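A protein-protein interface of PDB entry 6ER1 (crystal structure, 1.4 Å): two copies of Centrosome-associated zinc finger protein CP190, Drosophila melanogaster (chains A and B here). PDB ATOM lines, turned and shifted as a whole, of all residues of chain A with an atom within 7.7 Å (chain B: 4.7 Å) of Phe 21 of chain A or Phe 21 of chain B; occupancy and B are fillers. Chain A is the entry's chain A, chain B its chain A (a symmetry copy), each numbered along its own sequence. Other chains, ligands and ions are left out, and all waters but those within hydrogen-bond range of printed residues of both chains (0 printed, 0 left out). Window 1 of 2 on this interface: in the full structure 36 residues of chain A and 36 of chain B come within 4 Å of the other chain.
The backbone carbonyl oxygen (O) of Met 93 of chain A is in hydrogen-bond range of the indole nitrogen (NE1) of Trp 17 of chain B.
A ring nitrogen (ND1) of His 50 of chain A is in hydrogen-bond range of the side-chain hydroxyl (OH) of Tyr 94 of chain A (2.6 Å).
Among the printed residues, merely in contact across the chains: Leu 22 of chain A with Gly 18 of chain B (3.3 Å), Gly 18 of chain A with Leu 22 of chain B (3.3 Å), Thr 95 of chain A with Trp 17 of chain B (3.4 Å), His 50 of chain A with Leu 52 of chain B (3.5 Å), Ala 56 of chain A with Lys 24 of chain B (3.6 Å), Lys 24 of chain A with Ala 56 of chain B (3.6 Å), Phe 28 of chain A with Leu 52 of chain B (3.6 Å), Phe 21 of chain A with Leu 52 of chain B (3.6 Å), Leu 52 of chain A with Phe 21 of chain B (3.6 Å), Phe 21 of chain A with Phe 21 of chain B (3.6 Å), Trp 17 of chain A with Leu 22 of chain B (3.7 Å), Leu 22 of chain A with Trp 17 of chain B (3.7 Å), Gly 18 of chain A with Gly 18 of chain B (3.8 Å), Cys 57 of chain A with Trp 17 of chain B (3.8 Å), Phe 20 of chain A with Ala 56 of chain B (3.8 Å), Ala 56 of chain A with Phe 20 of chain B (3.8 Å), Leu 52 of chain A with Leu 52 of chain B (3.8 Å), Phe 28 of chain A with Ala 56 of chain B (3.8 Å), Leu 25 of chain A with Leu 52 of chain B (3.9 Å), Leu 52 of chain A with Leu 25 of chain B (3.9 Å), Ala 56 of chain A with Phe 21 of chain B (3.9 Å), Phe 21 of chain A with Ala 56 of chain B (3.9 Å), Val 53 of chain A with Phe 21 of chain B (3.9 Å) and Phe 21 of chain A with Val 53 of chain B (3.9 Å).
Of the printed residues of chain B, Leu 52 of chain A touches Phe 21, Leu 25 and Leu 52.
Printed residues of chain B within 4 Å of Val 53 of chain A: Phe 21 (3.9 Å).
Printed residues of chain B within 4 Å of Cys 57 of chain A: Trp 17 (3.8 Å).
Tyr 94 of chain A touches none of the printed residues of chain B.
Of the printed residues of chain B, Thr 95 of chain A touches Trp 17.
Printed residues of chain A within 4 Å of Trp 17 of chain B: Leu 22, Cys 57, Met 93 and Thr 95.
Phe 21 of chain B touches just these residues of chain A: Phe 21 (3.6 Å), Leu 52 (3.6 Å), Val 53 (3.9 Å) and Ala 56 (3.9 Å).
The nearest residue of chain B that does not touch Phe 21 of chain A is Leu 25 of chain B (4.1 Å).
The nearest printed residue of chain B that does not touch Gly 18 of chain A is Val 19 of chain B (4.5 Å).
Hydrophobic or aromatic side chains of chain B that line the printed part of chain A: Trp 17, Phe 20, Phe 21, Leu 22, Leu 25, Leu 52 and Ala 56.
Of the 23 printed residues of chain A, 15 touch a printed residue of chain B.
Hydrophobic or aromatic side chains of chain A within 4 Å of the printed part of chain B: Trp 17, Phe 20, Phe 21, Leu 22, Leu 25, Phe 28, His 50, Leu 52 and Ala 56.
Trp 17 of chain A touches Leu 22 of chain B, and with the chains exchanged Leu 22 of chain A touches Trp 17 of chain B.
Gly 18 of chain B touches its own counterpart, Gly 18 of chain A.
Phe 21 of chain A touches its own counterpart, Phe 21 of chain B.
Phe 21 of chain A touches Ala 56 of chain B, and with the chains exchanged Ala 56 of chain A touches Phe 21 of chain B.
Of the 25 pairs that touch across the chains among the printed residues, 19 have their exchanged pair printed and touching as well.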
ATOM      1  N   ASN A  16      21.439  -2.887   9.960  1.00  0.00           N
ATOM      2  CA  ASN A  16      21.788  -4.155   9.315  1.00  0.00           C
ATOM      3  C   ASN A  16      22.566  -5.087  10.241  1.00  0.00           C
ATOM      4  O   ASN A  16      23.547  -5.734   9.846  1.00  0.00           O
ATOM      5  CB  ASN A  16      22.541  -3.922   7.997  1.00  0.00           C
ATOM      6  CG  ASN A  16      21.768  -3.039   7.047  1.00  0.00           C
ATOM      7  OD1 ASN A  16      20.623  -3.329   6.738  1.00  0.00           O
ATOM      8  ND2 ASN A  16      22.375  -1.948   6.602  1.00  0.00           N
ATOM      9  N   TRP A  17      22.078  -5.190  11.473  1.00  0.00           N
ATOM     10  CA  TRP A  17      22.764  -6.017  12.466  1.00  0.00           C
ATOM     11  C   TRP A  17      22.865  -7.483  12.057  1.00  0.00           C
ATOM     12  O   TRP A  17      23.871  -8.150  12.335  1.00  0.00           O
ATOM     13  CB  TRP A  17      22.061  -5.915  13.841  1.00  0.00           C
ATOM     14  CG  TRP A  17      22.885  -6.479  14.946  1.00  0.00           C
ATOM     15  CD1 TRP A  17      22.601  -7.525  15.742  1.00  0.00           C
ATOM     16  CD2 TRP A  17      24.140  -5.971  15.388  1.00  0.00           C
ATOM     17  NE1 TRP A  17      23.622  -7.740  16.635  1.00  0.00           N
ATOM     18  CE2 TRP A  17      24.566  -6.777  16.452  1.00  0.00           C
ATOM     19  CE3 TRP A  17      24.935  -4.880  15.004  1.00  0.00           C
ATOM     20  CZ2 TRP A  17      25.736  -6.521  17.154  1.00  0.00           C
ATOM     21  CZ3 TRP A  17      26.076  -4.621  15.716  1.00  0.00           C
ATOM     22  CH2 TRP A  17      26.477  -5.446  16.762  1.00  0.00           C
ATOM     23  N   GLY A  18      21.830  -7.978  11.393  1.00  0.00           N
ATOM     24  CA  GLY A  18      21.818  -9.351  10.937  1.00  0.00           C
ATOM     25  C   GLY A  18      22.969  -9.684   9.996  1.00  0.00           C
ATOM     26  O   GLY A  18      23.540 -10.741  10.088  1.00  0.00           O
ATOM     27  N   VAL A  19      23.273  -8.761   9.082  1.00  0.00           N
ATOM     28  CA  VAL A  19      24.375  -8.901   8.131  1.00  0.00           C
ATOM     29  C   VAL A  19      25.704  -8.912   8.884  1.00  0.00           C
ATOM     30  O   VAL A  19      26.561  -9.793   8.633  1.00  0.00           O
ATOM     31  CB  VAL A  19      24.290  -7.764   7.069  1.00  0.00           C
ATOM     32  CG1 VAL A  19      25.487  -7.752   6.160  1.00  0.00           C
ATOM     33  CG2 VAL A  19      22.999  -7.865   6.265  1.00  0.00           C
ATOM     34  N   PHE A  20      25.863  -7.965   9.827  1.00  0.00           N
ATOM     35  CA  PHE A  20      27.059  -7.938  10.697  1.00  0.00           C
ATOM     36  C   PHE A  20      27.262  -9.289  11.405  1.00  0.00           C
ATOM     37  O   PHE A  20      28.344  -9.870  11.382  1.00  0.00           O
ATOM     38  CB  PHE A  20      26.955  -6.771  11.693  1.00  0.00           C
ATOM     39  CG  PHE A  20      27.990  -6.804  12.810  1.00  0.00           C
ATOM     40  CD1 PHE A  20      29.255  -6.298  12.622  1.00  0.00           C
ATOM     41  CD2 PHE A  20      27.703  -7.407  14.024  1.00  0.00           C
ATOM     42  CE1 PHE A  20      30.207  -6.363  13.625  1.00  0.00           C
ATOM     43  CE2 PHE A  20      28.658  -7.516  15.022  1.00  0.00           C
ATOM     44  CZ  PHE A  20      29.900  -6.976  14.833  1.00  0.00           C
ATOM     45  N   PHE A  21      26.206  -9.773  12.039  1.00  0.00           N
ATOM     46  CA  PHE A  21      26.289 -10.924  12.876  1.00  0.00           C
ATOM     47  C   PHE A  21      26.587 -12.200  12.081  1.00  0.00           C
ATOM     48  O   PHE A  21      27.429 -12.999  12.489  1.00  0.00           O
ATOM     49  CB  PHE A  21      25.005 -11.111  13.705  1.00  0.00           C
ATOM     50  CG  PHE A  21      25.116 -12.242  14.660  1.00  0.00           C
ATOM     51  CD1 PHE A  21      25.775 -12.071  15.864  1.00  0.00           C
ATOM     52  CD2 PHE A  21      24.658 -13.509  14.307  1.00  0.00           C
ATOM     53  CE1 PHE A  21      25.952 -13.128  16.722  1.00  0.00           C
ATOM     54  CE2 PHE A  21      24.851 -14.570  15.160  1.00  0.00           C
ATOM     55  CZ  PHE A  21      25.499 -14.375  16.359  1.00  0.00           C
ATOM     56  N   LEU A  22      25.902 -12.355  10.951  1.00  0.00           N
ATOM     57  CA  LEU A  22      26.110 -13.502  10.094  1.00  0.00           C
ATOM     58  C   LEU A  22      27.552 -13.598   9.615  1.00  0.00           C
ATOM     59  O   LEU A  22      28.102 -14.694   9.527  1.00  0.00           O
ATOM     60  CB  LEU A  22      25.118 -13.542   8.946  1.00  0.00           C
ATOM     61  CG  LEU A  22      23.714 -14.015   9.261  1.00  0.00           C
ATOM     62  CD1 LEU A  22      22.835 -13.956   8.018  1.00  0.00           C
ATOM     63  CD2 LEU A  22      23.697 -15.398   9.882  1.00  0.00           C
ATOM     64  N   GLN A  23      28.164 -12.461   9.294  1.00  0.00           N
ATOM     65  CA  GLN A  23      29.560 -12.489   8.850  1.00  0.00           C
ATOM     66  C   GLN A  23      30.440 -13.075   9.935  1.00  0.00           C
ATOM     67  O   GLN A  23      31.353 -13.884   9.682  1.00  0.00           O
ATOM     68  CB  GLN A  23      30.019 -11.094   8.448  1.00  0.00           C
ATOM     69  CG  GLN A  23      31.365 -11.041   7.723  1.00  0.00           C
ATOM     70  CD  GLN A  23      32.611 -10.896   8.623  1.00  0.00           C
ATOM     71  OE1 GLN A  23      33.656 -11.486   8.321  1.00  0.00           O
ATOM     72  NE2 GLN A  23      32.531 -10.084   9.685  1.00  0.00           N
ATOM     73  N   LYS A  24      30.173 -12.651  11.185  1.00  0.00           N
ATOM     74  CA  LYS A  24      30.963 -13.159  12.317  1.00  0.00           C
ATOM     75  C   LYS A  24      30.729 -14.632  12.573  1.00  0.00           C
ATOM     76  O   LYS A  24      31.678 -15.417  12.786  1.00  0.00           O
ATOM     77  CB  LYS A  24      30.657 -12.352  13.598  1.00  0.00           C
ATOM     78  CG  LYS A  24      30.988 -10.869  13.516  1.00  0.00           C
ATOM     79  CD  LYS A  24      32.473 -10.615  13.418  1.00  0.00           C
ATOM     80  CE  LYS A  24      32.813  -9.146  13.301  1.00  0.00           C
ATOM     81  NZ  LYS A  24      34.286  -8.979  13.153  1.00  0.00           N
ATOM     82  N   LEU A  25      29.467 -15.039  12.507  1.00  0.00           N
ATOM     83  CA  LEU A  25      29.096 -16.417  12.712  1.00  0.00           C
ATOM     84  C   LEU A  25      29.708 -17.359  11.636  1.00  0.00           C
ATOM     85  O   LEU A  25      30.191 -18.438  11.946  1.00  0.00           O
ATOM     86  CB  LEU A  25      27.582 -16.556  12.633  1.00  0.00           C
ATOM     87  CG  LEU A  25      26.963 -17.920  12.832  1.00  0.00           C
ATOM     88  CD1 LEU A  25      27.173 -18.439  14.250  1.00  0.00           C
ATOM     89  CD2 LEU A  25      25.490 -17.932  12.396  1.00  0.00           C
ATOM     90  N   GLN A  26      29.669 -16.915  10.398  1.00  0.00           N
ATOM     91  CA  GLN A  26      30.254 -17.698   9.277  1.00  0.00           C
ATOM     92  C   GLN A  26      31.742 -17.892   9.493  1.00  0.00           C
ATOM     93  O   GLN A  26      32.261 -18.997   9.298  1.00  0.00           O
ATOM     94  CB  GLN A  26      29.930 -16.976   8.000  1.00  0.00           C
ATOM     95  CG  GLN A  26      28.491 -17.181   7.604  1.00  0.00           C
ATOM     96  CD  GLN A  26      28.003 -16.174   6.599  1.00  0.00           C
ATOM     97  OE1 GLN A  26      28.797 -15.464   5.967  1.00  0.00           O
ATOM     98  NE2 GLN A  26      26.695 -16.133   6.407  1.00  0.00           N
ATOM     99  N   ASN A  27      32.439 -16.841   9.933  1.00  0.00           N
ATOM    100  CA  ASN A  27      33.833 -16.967  10.271  1.00  0.00           C
ATOM    101  C   ASN A  27      34.083 -17.980  11.369  1.00  0.00           C
ATOM    102  O   ASN A  27      35.000 -18.783  11.303  1.00  0.00           O
ATOM    103  CB  ASN A  27      34.429 -15.614  10.601  1.00  0.00           C
ATOM    104  CG  ASN A  27      35.900 -15.691  10.946  1.00  0.00           C
ATOM    105  OD1 ASN A  27      36.712 -16.098  10.094  1.00  0.00           O
ATOM    106  ND2 ASN A  27      36.252 -15.325  12.180  1.00  0.00           N
ATOM    107  N   PHE A  28      33.269 -17.937  12.412  1.00  0.00           N
ATOM    108  CA  PHE A  28      33.404 -18.932  13.465  1.00  0.00           C
ATOM    109  C   PHE A  28      33.224 -20.387  12.958  1.00  0.00           C
ATOM    110  O   PHE A  28      33.913 -21.313  13.404  1.00  0.00           O
ATOM    111  CB  PHE A  28      32.409 -18.670  14.596  1.00  0.00           C
ATOM    112  CG  PHE A  28      32.635 -17.383  15.361  1.00  0.00           C
ATOM    113  CD1 PHE A  28      33.905 -16.799  15.498  1.00  0.00           C
ATOM    114  CD2 PHE A  28      31.543 -16.752  15.914  1.00  0.00           C
ATOM    115  CE1 PHE A  28      34.065 -15.629  16.215  1.00  0.00           C
ATOM    116  CE2 PHE A  28      31.697 -15.602  16.663  1.00  0.00           C
ATOM    117  CZ  PHE A  28      32.944 -15.033  16.793  1.00  0.00           C
ATOM    118  N   HIS A  50      27.441 -25.384  15.254  1.00  0.00           N
ATOM    119  CA  HIS A  50      26.824 -24.727  16.432  1.00  0.00           C
ATOM    120  C   HIS A  50      25.398 -25.180  16.565  1.00  0.00           C
ATOM    121  O   HIS A  50      24.586 -24.922  15.675  1.00  0.00           O
ATOM    122  CB  HIS A  50      26.863 -23.222  16.292  1.00  0.00           C
ATOM    123  CG  HIS A  50      28.225 -22.653  16.077  1.00  0.00           C
ATOM    124  ND1 HIS A  50      28.720 -22.393  14.809  1.00  0.00           N
ATOM    125  CD2 HIS A  50      29.221 -22.334  16.940  1.00  0.00           C
ATOM    126  CE1 HIS A  50      29.941 -21.917  14.901  1.00  0.00           C
ATOM    127  NE2 HIS A  50      30.280 -21.877  16.183  1.00  0.00           N
ATOM    128  N   LEU A  52      22.915 -24.020  18.204  1.00  0.00           N
ATOM    129  CA  LEU A  52      21.918 -22.977  18.108  1.00  0.00           C
ATOM    130  C   LEU A  52      21.639 -22.579  16.677  1.00  0.00           C
ATOM    131  O   LEU A  52      20.495 -22.184  16.369  1.00  0.00           O
ATOM    132  CB  LEU A  52      22.310 -21.809  18.975  1.00  0.00           C
ATOM    133  CG  LEU A  52      23.297 -20.741  18.575  1.00  0.00           C
ATOM    134  CD1 LEU A  52      22.712 -19.833  17.498  1.00  0.00           C
ATOM    135  CD2 LEU A  52      23.695 -19.870  19.754  1.00  0.00           C
ATOM    136  N   VAL A  53      22.657 -22.682  15.785  1.00  0.00           N
ATOM    137  CA  VAL A  53      22.400 -22.331  14.396  1.00  0.00           C
ATOM    138  C   VAL A  53      21.457 -23.364  13.766  1.00  0.00           C
ATOM    139  O   VAL A  53      20.505 -23.028  13.032  1.00  0.00           O
ATOM    140  CB  VAL A  53      23.722 -22.250  13.610  1.00  0.00           C
ATOM    141  CG1 VAL A  53      23.441 -21.997  12.146  1.00  0.00           C
ATOM    142  CG2 VAL A  53      24.570 -21.099  14.167  1.00  0.00           C
ATOM    143  N   LEU A  54      21.744 -24.627  14.028  1.00  0.00           N
ATOM    144  CA  LEU A  54      20.914 -25.719  13.486  1.00  0.00           C
ATOM    145  C   LEU A  54      19.463 -25.585  14.012  1.00  0.00           C
ATOM    146  O   LEU A  54      18.453 -25.682  13.271  1.00  0.00           O
ATOM    147  CB  LEU A  54      21.518 -27.065  13.857  1.00  0.00           C
ATOM    148  CG  LEU A  54      22.622 -27.574  12.861  1.00  0.00           C
ATOM    149  CD1 LEU A  54      23.655 -26.585  12.458  1.00  0.00           C
ATOM    150  CD2 LEU A  54      23.322 -28.783  13.430  1.00  0.00           C
ATOM    151  N   SER A  55      19.364 -25.230  15.274  1.00  0.00           N
ATOM    152  CA  SER A  55      18.051 -25.165  15.948  1.00  0.00           C
ATOM    153  C   SER A  55      17.161 -24.013  15.448  1.00  0.00           C
ATOM    154  O   SER A  55      15.939 -24.070  15.587  1.00  0.00           O
ATOM    155  CB  SER A  55      18.200 -25.041  17.443  1.00  0.00           C
ATOM    156  OG  SER A  55      18.960 -26.139  17.979  1.00  0.00           O
ATOM    157  N   ALA A  56      17.759 -22.985  14.851  1.00  0.00           N
ATOM    158  CA  ALA A  56      16.950 -21.872  14.302  1.00  0.00           C
ATOM    159  C   ALA A  56      16.050 -22.330  13.148  1.00  0.00           C
ATOM    160  O   ALA A  56      15.033 -21.697  12.879  1.00  0.00           O
ATOM    161  CB  ALA A  56      17.850 -20.769  13.819  1.00  0.00           C
ATOM    162  N   CYS A  57      16.511 -23.386  12.458  1.00  0.00           N
ATOM    163  CA  CYS A  57      15.806 -23.907  11.260  1.00  0.00           C
ATOM    164  C   CYS A  57      15.023 -25.170  11.451  1.00  0.00           C
ATOM    165  O   CYS A  57      14.112 -25.490  10.633  1.00  0.00           O
ATOM    166  CB  CYS A  57      16.766 -24.157  10.095  1.00  0.00           C
ATOM    167  SG  CYS A  57      17.383 -22.634   9.375  1.00  0.00           S
ATOM    168  N   MET A  93      21.887 -23.271   6.452  1.00  0.00           N
ATOM    169  CA  MET A  93      21.507 -22.723   7.790  1.00  0.00           C
ATOM    170  C   MET A  93      22.378 -21.559   8.196  1.00  0.00           C
ATOM    171  O   MET A  93      21.896 -20.599   8.859  1.00  0.00           O
ATOM    172  CB  MET A  93      21.577 -23.796   8.846  1.00  0.00           C
ATOM    173  CG  MET A  93      20.585 -24.877   8.662  1.00  0.00           C
ATOM    174  SD  MET A  93      21.036 -26.271   9.720  1.00  0.00           S
ATOM    175  CE  MET A  93      19.589 -27.039   9.837  1.00  0.00           C
ATOM    176  N   TYR A  94      23.647 -21.537   7.805  1.00  0.00           N
ATOM    177  CA  TYR A  94      24.582 -20.443   8.124  1.00  0.00           C
ATOM    178  C   TYR A  94      24.465 -19.221   7.224  1.00  0.00           C
ATOM    179  O   TYR A  94      24.866 -18.114   7.612  1.00  0.00           O
ATOM    180  CB  TYR A  94      26.026 -20.918   8.117  1.00  0.00           C
ATOM    181  CG  TYR A  94      26.433 -21.671   9.364  1.00  0.00           C
ATOM    182  CD1 TYR A  94      26.208 -23.019   9.515  1.00  0.00           C
ATOM    183  CD2 TYR A  94      27.001 -20.990  10.445  1.00  0.00           C
ATOM    184  CE1 TYR A  94      26.544 -23.695  10.673  1.00  0.00           C
ATOM    185  CE2 TYR A  94      27.349 -21.657  11.600  1.00  0.00           C
ATOM    186  CZ  TYR A  94      27.112 -23.008  11.731  1.00  0.00           C
ATOM    187  OH  TYR A  94      27.491 -23.689  12.854  1.00  0.00           O
ATOM    188  N   THR A  95      23.881 -19.387   6.052  1.00  0.00           N
ATOM    189  CA  THR A  95      23.969 -18.347   5.028  1.00  0.00           C
ATOM    190  C   THR A  95      22.686 -17.869   4.380  1.00  0.00           C
ATOM    191  O   THR A  95      22.654 -16.732   3.888  1.00  0.00           O
ATOM    192  CB  THR A  95      24.885 -18.778   3.844  1.00  0.00           C
ATOM    193  OG1 THR A  95      24.298 -19.861   3.143  1.00  0.00           O
ATOM    194  CG2 THR A  95      26.276 -19.162   4.295  1.00  0.00           C
ATOM    195  N   TRP B  17      18.462 -13.141   5.258  1.00  0.00           N
ATOM    196  CA  TRP B  17      18.713 -14.242   6.188  1.00  0.00           C
ATOM    197  C   TRP B  17      19.094 -13.771   7.587  1.00  0.00           C
ATOM    198  O   TRP B  17      18.713 -14.388   8.590  1.00  0.00           O
ATOM    199  CB  TRP B  17      19.820 -15.176   5.642  1.00  0.00           C
ATOM    200  CG  TRP B  17      19.896 -16.465   6.384  1.00  0.00           C
ATOM    201  CD1 TRP B  17      20.921 -16.946   7.110  1.00  0.00           C
ATOM    202  CD2 TRP B  17      18.877 -17.459   6.426  1.00  0.00           C
ATOM    203  NE1 TRP B  17      20.597 -18.167   7.648  1.00  0.00           N
ATOM    204  CE2 TRP B  17      19.354 -18.514   7.217  1.00  0.00           C
ATOM    205  CE3 TRP B  17      17.608 -17.575   5.838  1.00  0.00           C
ATOM    206  CZ2 TRP B  17      18.626 -19.677   7.420  1.00  0.00           C
ATOM    207  CZ3 TRP B  17      16.905 -18.735   6.025  1.00  0.00           C
ATOM    208  CH2 TRP B  17      17.402 -19.760   6.823  1.00  0.00           C
ATOM    209  N   GLY B  18      19.838 -12.674   7.652  1.00  0.00           N
ATOM    210  CA  GLY B  18      20.248 -12.120   8.925  1.00  0.00           C
ATOM    211  C   GLY B  18      19.076 -11.746   9.824  1.00  0.00           C
ATOM    212  O   GLY B  18      19.126 -11.968  11.008  1.00  0.00           O
ATOM    213  N   VAL B  19      18.037 -11.156   9.230  1.00  0.00           N
ATOM    214  CA  VAL B  19      16.817 -10.772   9.938  1.00  0.00           C
ATOM    215  C   VAL B  19      16.101 -12.023  10.443  1.00  0.00           C
ATOM    216  O   VAL B  19      15.700 -12.081  11.630  1.00  0.00           O
ATOM    217  CB  VAL B  19      15.927  -9.902   9.000  1.00  0.00           C
ATOM    218  CG1 VAL B  19      14.584  -9.611   9.608  1.00  0.00           C
ATOM    219  CG2 VAL B  19      16.640  -8.610   8.617  1.00  0.00           C
ATOM    220  N   PHE B  20      15.972 -13.033   9.562  1.00  0.00           N
ATOM    221  CA  PHE B  20      15.396 -14.334   9.963  1.00  0.00           C
ATOM    222  C   PHE B  20      16.132 -14.917  11.182  1.00  0.00           C
ATOM    223  O   PHE B  20      15.522 -15.308  12.174  1.00  0.00           O
ATOM    224  CB  PHE B  20      15.402 -15.299   8.766  1.00  0.00           C
ATOM    225  CG  PHE B  20      15.085 -16.746   9.124  1.00  0.00           C
ATOM    226  CD1 PHE B  20      13.786 -17.181   9.241  1.00  0.00           C
ATOM    227  CD2 PHE B  20      16.102 -17.645   9.407  1.00  0.00           C
ATOM    228  CE1 PHE B  20      13.500 -18.487   9.604  1.00  0.00           C
ATOM    229  CE2 PHE B  20      15.830 -18.941   9.810  1.00  0.00           C
ATOM    230  CZ  PHE B  20      14.533 -19.370   9.887  1.00  0.00           C
ATOM    231  N   PHE B  21      17.451 -14.974  11.087  1.00  0.00           N
ATOM    232  CA  PHE B  21      18.250 -15.640  12.062  1.00  0.00           C
ATOM    233  C   PHE B  21      18.226 -14.928  13.419  1.00  0.00           C
ATOM    234  O   PHE B  21      18.088 -15.577  14.455  1.00  0.00           O
ATOM    235  CB  PHE B  21      19.704 -15.803  11.582  1.00  0.00           C
ATOM    236  CG  PHE B  21      20.524 -16.588  12.538  1.00  0.00           C
ATOM    237  CD1 PHE B  21      20.453 -17.970  12.539  1.00  0.00           C
ATOM    238  CD2 PHE B  21      21.284 -15.943  13.510  1.00  0.00           C
ATOM    239  CE1 PHE B  21      21.146 -18.705  13.469  1.00  0.00           C
ATOM    240  CE2 PHE B  21      21.964 -16.681  14.450  1.00  0.00           C
ATOM    241  CZ  PHE B  21      21.889 -18.055  14.426  1.00  0.00           C
ATOM    242  N   LEU B  22      18.342 -13.603  13.383  1.00  0.00           N
ATOM    243  CA  LEU B  22      18.306 -12.809  14.592  1.00  0.00           C
ATOM    244  C   LEU B  22      17.003 -12.999  15.356  1.00  0.00           C
ATOM    245  O   LEU B  22      17.010 -13.047  16.585  1.00  0.00           O
ATOM    246  CB  LEU B  22      18.607 -11.346  14.321  1.00  0.00           C
ATOM    247  CG  LEU B  22      20.056 -10.967  14.101  1.00  0.00           C
ATOM    248  CD1 LEU B  22      20.184  -9.479  13.801  1.00  0.00           C
ATOM    249  CD2 LEU B  22      20.942 -11.373  15.262  1.00  0.00           C
ATOM    250  N   GLN B  23      15.886 -13.096  14.640  1.00  0.00           N
ATOM    251  CA  GLN B  23      14.605 -13.304  15.319  1.00  0.00           C
ATOM    252  C   GLN B  23      14.638 -14.597  16.107  1.00  0.00           C
ATOM    253  O   GLN B  23      14.160 -14.686  17.255  1.00  0.00           O
ATOM    254  CB  GLN B  23      13.460 -13.289  14.315  1.00  0.00           C
ATOM    255  CG  GLN B  23      12.061 -13.232  14.931  1.00  0.00           C
ATOM    256  CD  GLN B  23      11.406 -14.594  15.245  1.00  0.00           C
ATOM    257  OE1 GLN B  23      10.709 -14.719  16.259  1.00  0.00           O
ATOM    258  NE2 GLN B  23      11.577 -15.593  14.369  1.00  0.00           N
ATOM    259  N   LYS B  24      15.206 -15.643  15.477  1.00  0.00           N
ATOM    260  CA  LYS B  24      15.296 -16.947  16.151  1.00  0.00           C
ATOM    261  C   LYS B  24      16.233 -16.922  17.339  1.00  0.00           C
ATOM    262  O   LYS B  24      15.920 -17.445  18.430  1.00  0.00           O
ATOM    263  CB  LYS B  24      15.742 -18.041  15.158  1.00  0.00           C
ATOM    264  CG  LYS B  24      14.800 -18.266  13.984  1.00  0.00           C
ATOM    265  CD  LYS B  24      13.475 -18.851  14.412  1.00  0.00           C
ATOM    266  CE  LYS B  24      12.517 -19.046  13.259  1.00  0.00           C
ATOM    267  NZ  LYS B  24      11.218 -19.572  13.766  1.00  0.00           N
ATOM    268  N   LEU B  25      17.377 -16.271  17.162  1.00  0.00           N
ATOM    269  CA  LEU B  25      18.359 -16.151  18.211  1.00  0.00           C
ATOM    270  C   LEU B  25      17.820 -15.359  19.436  1.00  0.00           C
ATOM    271  O   LEU B  25      18.044 -15.735  20.577  1.00  0.00           O
ATOM    272  CB  LEU B  25      19.579 -15.406  17.686  1.00  0.00           C
ATOM    273  CG  LEU B  25      20.748 -15.174  18.615  1.00  0.00           C
ATOM    274  CD1 LEU B  25      21.425 -16.480  19.017  1.00  0.00           C
ATOM    275  CD2 LEU B  25      21.725 -14.141  18.034  1.00  0.00           C
ATOM    276  N   LEU B  52      28.930 -17.586  21.728  1.00  0.00           N
ATOM    277  CA  LEU B  52      29.220 -17.173  20.373  1.00  0.00           C
ATOM    278  C   LEU B  52      28.645 -15.813  20.051  1.00  0.00           C
ATOM    279  O   LEU B  52      29.241 -15.080  19.234  1.00  0.00           O
ATOM    280  CB  LEU B  52      28.779 -18.240  19.404  1.00  0.00           C
ATOM    281  CG  LEU B  52      27.361 -18.422  18.922  1.00  0.00           C
ATOM    282  CD1 LEU B  52      26.959 -17.297  17.972  1.00  0.00           C
ATOM    283  CD2 LEU B  52      27.180 -19.739  18.187  1.00  0.00           C
ATOM    284  N   VAL B  53      27.500 -15.449  20.682  1.00  0.00           N
ATOM    285  CA  VAL B  53      26.947 -14.130  20.408  1.00  0.00           C
ATOM    286  C   VAL B  53      27.866 -13.050  20.990  1.00  0.00           C
ATOM    287  O   VAL B  53      28.152 -12.013  20.357  1.00  0.00           O
ATOM    288  CB  VAL B  53      25.528 -14.012  20.995  1.00  0.00           C
ATOM    289  CG1 VAL B  53      25.003 -12.606  20.806  1.00  0.00           C
ATOM    290  CG2 VAL B  53      24.600 -14.998  20.274  1.00  0.00           C
ATOM    291  N   ALA B  56      31.087 -12.448  18.928  1.00  0.00           N
ATOM    292  CA  ALA B  56      31.002 -11.719  17.641  1.00  0.00           C
ATOM    293  C   ALA B  56      31.410 -10.248  17.785  1.00  0.00           C
ATOM    294  O   ALA B  56      31.819  -9.629  16.806  1.00  0.00           O
ATOM    295  CB  ALA B  56      29.602 -11.792  17.097  1.00  0.00           C
